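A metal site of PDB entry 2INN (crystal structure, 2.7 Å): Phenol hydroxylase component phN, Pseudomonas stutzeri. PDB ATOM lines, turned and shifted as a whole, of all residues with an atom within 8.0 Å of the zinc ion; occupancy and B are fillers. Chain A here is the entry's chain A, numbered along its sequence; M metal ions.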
ATOM      1  N   TRP A 267      32.421   2.616 -22.072  1.00  0.00           N
ATOM      2  CA  TRP A 267      32.166   3.998 -22.383  1.00  0.00           C
ATOM      3  C   TRP A 267      30.747   4.125 -22.868  1.00  0.00           C
ATOM      4  O   TRP A 267      30.038   4.928 -22.378  1.00  0.00           O
ATOM      5  CB  TRP A 267      33.213   4.623 -23.300  1.00  0.00           C
ATOM      6  CG  TRP A 267      32.921   6.071 -23.546  1.00  0.00           C
ATOM      7  CD1 TRP A 267      32.196   6.610 -24.588  1.00  0.00           C
ATOM      8  CD2 TRP A 267      33.293   7.194 -22.711  1.00  0.00           C
ATOM      9  NE1 TRP A 267      32.130   7.981 -24.468  1.00  0.00           N
ATOM     10  CE2 TRP A 267      32.774   8.377 -23.327  1.00  0.00           C
ATOM     11  CE3 TRP A 267      33.973   7.307 -21.499  1.00  0.00           C
ATOM     12  CZ2 TRP A 267      32.925   9.637 -22.773  1.00  0.00           C
ATOM     13  CZ3 TRP A 267      34.130   8.587 -20.947  1.00  0.00           C
ATOM     14  CH2 TRP A 267      33.591   9.725 -21.572  1.00  0.00           C
ATOM     15  N   ARG A 268      30.302   3.283 -23.776  1.00  0.00           N
ATOM     16  CA  ARG A 268      28.901   3.208 -24.099  1.00  0.00           C
ATOM     17  C   ARG A 268      28.088   3.070 -22.826  1.00  0.00           C
ATOM     18  O   ARG A 268      27.145   3.804 -22.666  1.00  0.00           O
ATOM     19  CB  ARG A 268      28.583   2.123 -25.123  1.00  0.00           C
ATOM     20  CG  ARG A 268      28.796   2.595 -26.558  1.00  0.00           C
ATOM     21  CD  ARG A 268      27.739   2.157 -27.628  1.00  0.00           C
ATOM     22  NE  ARG A 268      26.529   3.000 -27.572  1.00  0.00           N
ATOM     23  CZ  ARG A 268      25.513   3.005 -28.445  1.00  0.00           C
ATOM     24  NH1 ARG A 268      25.556   2.247 -29.531  1.00  0.00           N
ATOM     25  NH2 ARG A 268      24.447   3.771 -28.226  1.00  0.00           N
ATOM     26  N   ARG A 271      27.789   6.193 -20.741  1.00  0.00           N
ATOM     27  CA  ARG A 271      26.948   7.163 -21.407  1.00  0.00           C
ATOM     28  C   ARG A 271      25.477   6.841 -21.238  1.00  0.00           C
ATOM     29  O   ARG A 271      24.707   7.747 -20.993  1.00  0.00           O
ATOM     30  CB  ARG A 271      27.279   7.277 -22.904  1.00  0.00           C
ATOM     31  CG  ARG A 271      28.349   8.287 -23.264  1.00  0.00           C
ATOM     32  CD  ARG A 271      28.208   9.593 -22.466  1.00  0.00           C
ATOM     33  NE  ARG A 271      29.070  10.653 -22.984  1.00  0.00           N
ATOM     34  CZ  ARG A 271      29.672  11.557 -22.199  1.00  0.00           C
ATOM     35  NH1 ARG A 271      29.549  11.444 -20.889  1.00  0.00           N
ATOM     36  NH2 ARG A 271      30.422  12.553 -22.731  1.00  0.00           N
ATOM     37  N   LEU A 398      22.970  15.777 -32.044  1.00  0.00           N
ATOM     38  CA  LEU A 398      23.163  14.450 -31.350  1.00  0.00           C
ATOM     39  C   LEU A 398      24.537  13.834 -31.552  1.00  0.00           C
ATOM     40  O   LEU A 398      25.161  14.130 -32.546  1.00  0.00           O
ATOM     41  CB  LEU A 398      22.140  13.398 -31.810  1.00  0.00           C
ATOM     42  CG  LEU A 398      20.651  13.675 -31.609  1.00  0.00           C
ATOM     43  CD1 LEU A 398      19.809  12.490 -32.112  1.00  0.00           C
ATOM     44  CD2 LEU A 398      20.328  14.093 -30.190  1.00  0.00           C
ATOM     45  N   CYS A 399      25.023  12.953 -30.655  1.00  0.00           N
ATOM     46  CA  CYS A 399      26.350  12.381 -30.839  1.00  0.00           C
ATOM     47  C   CYS A 399      26.242  11.159 -31.761  1.00  0.00           C
ATOM     48  O   CYS A 399      25.369  10.315 -31.533  1.00  0.00           O
ATOM     49  CB  CYS A 399      26.946  11.975 -29.480  1.00  0.00           C
ATOM     50  SG  CYS A 399      28.514  10.989 -29.704  1.00  0.00           S
ATOM     51  N   GLN A 400      27.092  11.042 -32.777  1.00  0.00           N
ATOM     52  CA  GLN A 400      26.965   9.899 -33.716  1.00  0.00           C
ATOM     53  C   GLN A 400      27.087   8.562 -32.993  1.00  0.00           C
ATOM     54  O   GLN A 400      26.462   7.561 -33.381  1.00  0.00           O
ATOM     55  CB  GLN A 400      27.996   9.967 -34.799  1.00  0.00           C
ATOM     56  CG  GLN A 400      27.770   9.023 -35.986  1.00  0.00           C
ATOM     57  CD  GLN A 400      26.618   9.452 -36.895  1.00  0.00           C
ATOM     58  OE1 GLN A 400      25.834   8.585 -37.356  1.00  0.00           O
ATOM     59  NE2 GLN A 400      26.471  10.810 -37.122  1.00  0.00           N
ATOM     60  N   VAL A 401      27.832   8.494 -31.901  1.00  0.00           N
ATOM     61  CA  VAL A 401      27.829   7.218 -31.186  1.00  0.00           C
ATOM     62  C   VAL A 401      26.764   7.075 -30.053  1.00  0.00           C
ATOM     63  O   VAL A 401      25.946   6.131 -30.148  1.00  0.00           O
ATOM     64  CB  VAL A 401      29.230   6.809 -30.734  1.00  0.00           C
ATOM     65  CG1 VAL A 401      29.237   5.303 -30.321  1.00  0.00           C
ATOM     66  CG2 VAL A 401      30.217   7.070 -31.867  1.00  0.00           C
ATOM     67  N   CYS A 402      26.801   7.934 -28.991  1.00  0.00           N
ATOM     68  CA  CYS A 402      25.930   7.652 -27.848  1.00  0.00           C
ATOM     69  C   CYS A 402      24.485   8.102 -28.053  1.00  0.00           C
ATOM     70  O   CYS A 402      23.554   7.646 -27.338  1.00  0.00           O
ATOM     71  CB  CYS A 402      26.465   8.211 -26.571  1.00  0.00           C
ATOM     72  SG  CYS A 402      27.065   9.775 -26.633  1.00  0.00           S
ATOM     73  N   GLN A 403      24.334   8.943 -29.095  1.00  0.00           N
ATOM     74  CA  GLN A 403      23.062   9.566 -29.530  1.00  0.00           C
ATOM     75  C   GLN A 403      22.464  10.527 -28.528  1.00  0.00           C
ATOM     76  O   GLN A 403      21.413  11.063 -28.736  1.00  0.00           O
ATOM     77  CB  GLN A 403      22.067   8.574 -30.108  1.00  0.00           C
ATOM     78  CG  GLN A 403      22.695   7.848 -31.268  1.00  0.00           C
ATOM     79  CD  GLN A 403      21.710   6.938 -31.993  1.00  0.00           C
ATOM     80  OE1 GLN A 403      20.533   7.171 -31.932  1.00  0.00           O
ATOM     81  NE2 GLN A 403      22.201   5.919 -32.692  1.00  0.00           N
ATOM     82  N   ILE A 404      23.188  10.787 -27.460  1.00  0.00           N
ATOM     83  CA  ILE A 404      22.773  11.778 -26.511  1.00  0.00           C
ATOM     84  C   ILE A 404      23.103  13.157 -27.099  1.00  0.00           C
ATOM     85  O   ILE A 404      24.080  13.289 -27.747  1.00  0.00           O
ATOM     86  CB  ILE A 404      23.617  11.646 -25.259  1.00  0.00           C
ATOM     87  CG1 ILE A 404      23.353  10.314 -24.554  1.00  0.00           C
ATOM     88  CG2 ILE A 404      23.303  12.803 -24.314  1.00  0.00           C
ATOM     89  CD1 ILE A 404      24.015  10.135 -23.126  1.00  0.00           C
ATOM     90  N   PRO A 405      22.327  14.223 -26.790  1.00  0.00           N
ATOM     91  CA  PRO A 405      22.833  15.527 -27.176  1.00  0.00           C
ATOM     92  C   PRO A 405      24.224  15.831 -26.661  1.00  0.00           C
ATOM     93  O   PRO A 405      24.592  15.410 -25.566  1.00  0.00           O
ATOM     94  CB  PRO A 405      21.852  16.465 -26.503  1.00  0.00           C
ATOM     95  CG  PRO A 405      20.632  15.684 -26.393  1.00  0.00           C
ATOM     96  CD  PRO A 405      21.024  14.320 -26.102  1.00  0.00           C
ATOM     97  N   THR A 406      24.999  16.566 -27.447  1.00  0.00           N
ATOM     98  CA  THR A 406      26.341  16.967 -27.064  1.00  0.00           C
ATOM     99  C   THR A 406      26.413  18.015 -25.945  1.00  0.00           C
ATOM    100  O   THR A 406      26.896  19.151 -26.111  1.00  0.00           O
ATOM    101  CB  THR A 406      27.285  17.297 -28.299  1.00  0.00           C
ATOM    102  OG1 THR A 406      26.748  18.364 -29.077  1.00  0.00           O
ATOM    103  CG2 THR A 406      27.416  16.078 -29.173  1.00  0.00           C
ATOM    104  N   PHE A 408      27.901  17.296 -22.949  1.00  0.00           N
ATOM    105  CA  PHE A 408      29.013  17.050 -22.098  1.00  0.00           C
ATOM    106  C   PHE A 408      30.234  17.974 -22.230  1.00  0.00           C
ATOM    107  O   PHE A 408      30.580  18.468 -23.317  1.00  0.00           O
ATOM    108  CB  PHE A 408      29.353  15.615 -22.260  1.00  0.00           C
ATOM    109  CG  PHE A 408      28.210  14.723 -22.023  1.00  0.00           C
ATOM    110  CD1 PHE A 408      27.755  13.889 -23.020  1.00  0.00           C
ATOM    111  CD2 PHE A 408      27.625  14.684 -20.763  1.00  0.00           C
ATOM    112  CE1 PHE A 408      26.676  12.973 -22.782  1.00  0.00           C
ATOM    113  CE2 PHE A 408      26.566  13.821 -20.475  1.00  0.00           C
ATOM    114  CZ  PHE A 408      26.064  12.967 -21.481  1.00  0.00           C
ATOM    115  N   HIS A 430      29.907  13.896 -35.807  1.00  0.00           N
ATOM    116  CA  HIS A 430      30.082  14.651 -34.598  1.00  0.00           C
ATOM    117  C   HIS A 430      29.929  13.764 -33.364  1.00  0.00           C
ATOM    118  O   HIS A 430      29.108  12.795 -33.340  1.00  0.00           O
ATOM    119  CB  HIS A 430      29.008  15.747 -34.625  1.00  0.00           C
ATOM    120  CG  HIS A 430      29.322  16.872 -35.570  1.00  0.00           C
ATOM    121  ND1 HIS A 430      30.100  17.966 -35.199  1.00  0.00           N
ATOM    122  CD2 HIS A 430      28.983  17.071 -36.871  1.00  0.00           C
ATOM    123  CE1 HIS A 430      30.209  18.788 -36.228  1.00  0.00           C
ATOM    124  NE2 HIS A 430      29.535  18.281 -37.245  1.00  0.00           N
ATOM    125  N   PHE A 431      30.664  14.146 -32.309  1.00  0.00           N
ATOM    126  CA  PHE A 431      30.850  13.322 -31.123  1.00  0.00           C
ATOM    127  C   PHE A 431      30.765  14.109 -29.846  1.00  0.00           C
ATOM    128  O   PHE A 431      31.323  15.229 -29.705  1.00  0.00           O
ATOM    129  CB  PHE A 431      32.221  12.569 -31.200  1.00  0.00           C
ATOM    130  CG  PHE A 431      32.332  11.750 -32.408  1.00  0.00           C
ATOM    131  CD1 PHE A 431      31.486  10.656 -32.573  1.00  0.00           C
ATOM    132  CD2 PHE A 431      33.104  12.181 -33.452  1.00  0.00           C
ATOM    133  CE1 PHE A 431      31.469   9.972 -33.754  1.00  0.00           C
ATOM    134  CE2 PHE A 431      33.117  11.533 -34.644  1.00  0.00           C
ATOM    135  CZ  PHE A 431      32.317  10.402 -34.811  1.00  0.00           C
ATOM    136  N   CYS A 432      30.096  13.482 -28.882  1.00  0.00           N
ATOM    137  CA  CYS A 432      30.038  14.007 -27.544  1.00  0.00           C
ATOM    138  C   CYS A 432      31.382  14.109 -26.809  1.00  0.00           C
ATOM    139  O   CYS A 432      31.464  14.853 -25.880  1.00  0.00           O
ATOM    140  CB  CYS A 432      29.083  13.112 -26.749  1.00  0.00           C
ATOM    141  SG  CYS A 432      29.842  11.753 -26.125  1.00  0.00           S
ATOM    142  N   SER A 433      32.432  13.383 -27.241  1.00  0.00           N
ATOM    143  CA  SER A 433      33.633  13.129 -26.374  1.00  0.00           C
ATOM    144  C   SER A 433      34.815  12.421 -27.080  1.00  0.00           C
ATOM    145  O   SER A 433      34.634  11.878 -28.146  1.00  0.00           O
ATOM    146  CB  SER A 433      33.173  12.228 -25.244  1.00  0.00           C
ATOM    147  OG  SER A 433      32.781  10.976 -25.812  1.00  0.00           O
ATOM    148  N   ASP A 434      35.998  12.368 -26.486  1.00  0.00           N
ATOM    149  CA  ASP A 434      37.062  11.465 -27.067  1.00  0.00           C
ATOM    150  C   ASP A 434      36.620  10.013 -27.158  1.00  0.00           C
ATOM    151  O   ASP A 434      36.680   9.418 -28.248  1.00  0.00           O
ATOM    152  CB  ASP A 434      38.454  11.641 -26.424  1.00  0.00           C
ATOM    153  CG  ASP A 434      39.043  13.073 -26.735  1.00  0.00           C
ATOM    154  OD1 ASP A 434      39.091  13.424 -27.983  1.00  0.00           O
ATOM    155  OD2 ASP A 434      39.432  13.855 -25.785  1.00  0.00           O
ATOM    156  N   GLY A 435      36.070   9.499 -26.041  1.00  0.00           N
ATOM    157  CA  GLY A 435      35.510   8.175 -25.991  1.00  0.00           C
ATOM    158  C   GLY A 435      34.562   7.867 -27.138  1.00  0.00           C
ATOM    159  O   GLY A 435      34.552   6.771 -27.685  1.00  0.00           O
ATOM    160  N   CYS A 436      33.687   8.809 -27.494  1.00  0.00           N
ATOM    161  CA  CYS A 436      32.655   8.483 -28.431  1.00  0.00           C
ATOM    162  C   CYS A 436      33.308   8.531 -29.769  1.00  0.00           C
ATOM    163  O   CYS A 436      33.089   7.669 -30.616  1.00  0.00           O
ATOM    164  CB  CYS A 436      31.511   9.422 -28.313  1.00  0.00           C
ATOM    165  SG  CYS A 436      30.278   8.731 -27.169  1.00  0.00           S
ATOM    166  N   CYS A 437      34.196   9.482 -29.924  1.00  0.00           N
ATOM    167  CA  CYS A 437      34.984   9.524 -31.114  1.00  0.00           C
ATOM    168  C   CYS A 437      35.820   8.215 -31.335  1.00  0.00           C
ATOM    169  O   CYS A 437      35.756   7.601 -32.446  1.00  0.00           O
ATOM    170  CB  CYS A 437      35.892  10.736 -31.018  1.00  0.00           C
ATOM    171  SG  CYS A 437      36.670  11.018 -32.581  1.00  0.00           S
ATOM    172  N   ILE A 439      35.398   5.214 -30.447  1.00  0.00           N
ATOM    173  CA  ILE A 439      34.528   4.119 -30.837  1.00  0.00           C
ATOM    174  C   ILE A 439      34.155   4.259 -32.297  1.00  0.00           C
ATOM    175  O   ILE A 439      34.014   3.251 -32.991  1.00  0.00           O
ATOM    176  CB  ILE A 439      33.252   4.036 -29.939  1.00  0.00           C
ATOM    177  CG1 ILE A 439      33.627   3.679 -28.491  1.00  0.00           C
ATOM    178  CG2 ILE A 439      32.207   3.006 -30.476  1.00  0.00           C
ATOM    179  CD1 ILE A 439      32.491   3.873 -27.505  1.00  0.00           C
HETATM  180 ZN    ZN M   1      28.623  10.185 -27.494  1.00  0.00          ZN
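The backbone NH (N) of Cys 436 lies within hydrogen-bond range of the side-chain hydroxyl (OG) of Ser 433 (2.9 Å).
The side-chain sulfur of Cys 436 lies close to the indole nitrogen of Trp 267, 3.4 Å away.
The side-chain sulfur of Cys 399 lies close to the backbone NH of Val 401 (3.4 Å).
N of Cys 399 is in hydrogen-bond range of O of Ile 404 (3.1 Å).
The side-chain sulfur of Cys 432 lies close to the side-chain hydroxyl of Ser 433 (3.1 Å).
SG of Cys 432 lies close to NE of Arg 271.
Of the 22 residues printed, 4 come within 4 Å of the zinc ion.
The nearest printed residue that does not touch the zinc ion is Val 401 (4.4 Å).
The zinc ion is bound by SG of Cys 402, SG of Cys 436, SG of Cys 399 and SG of Cys 432.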
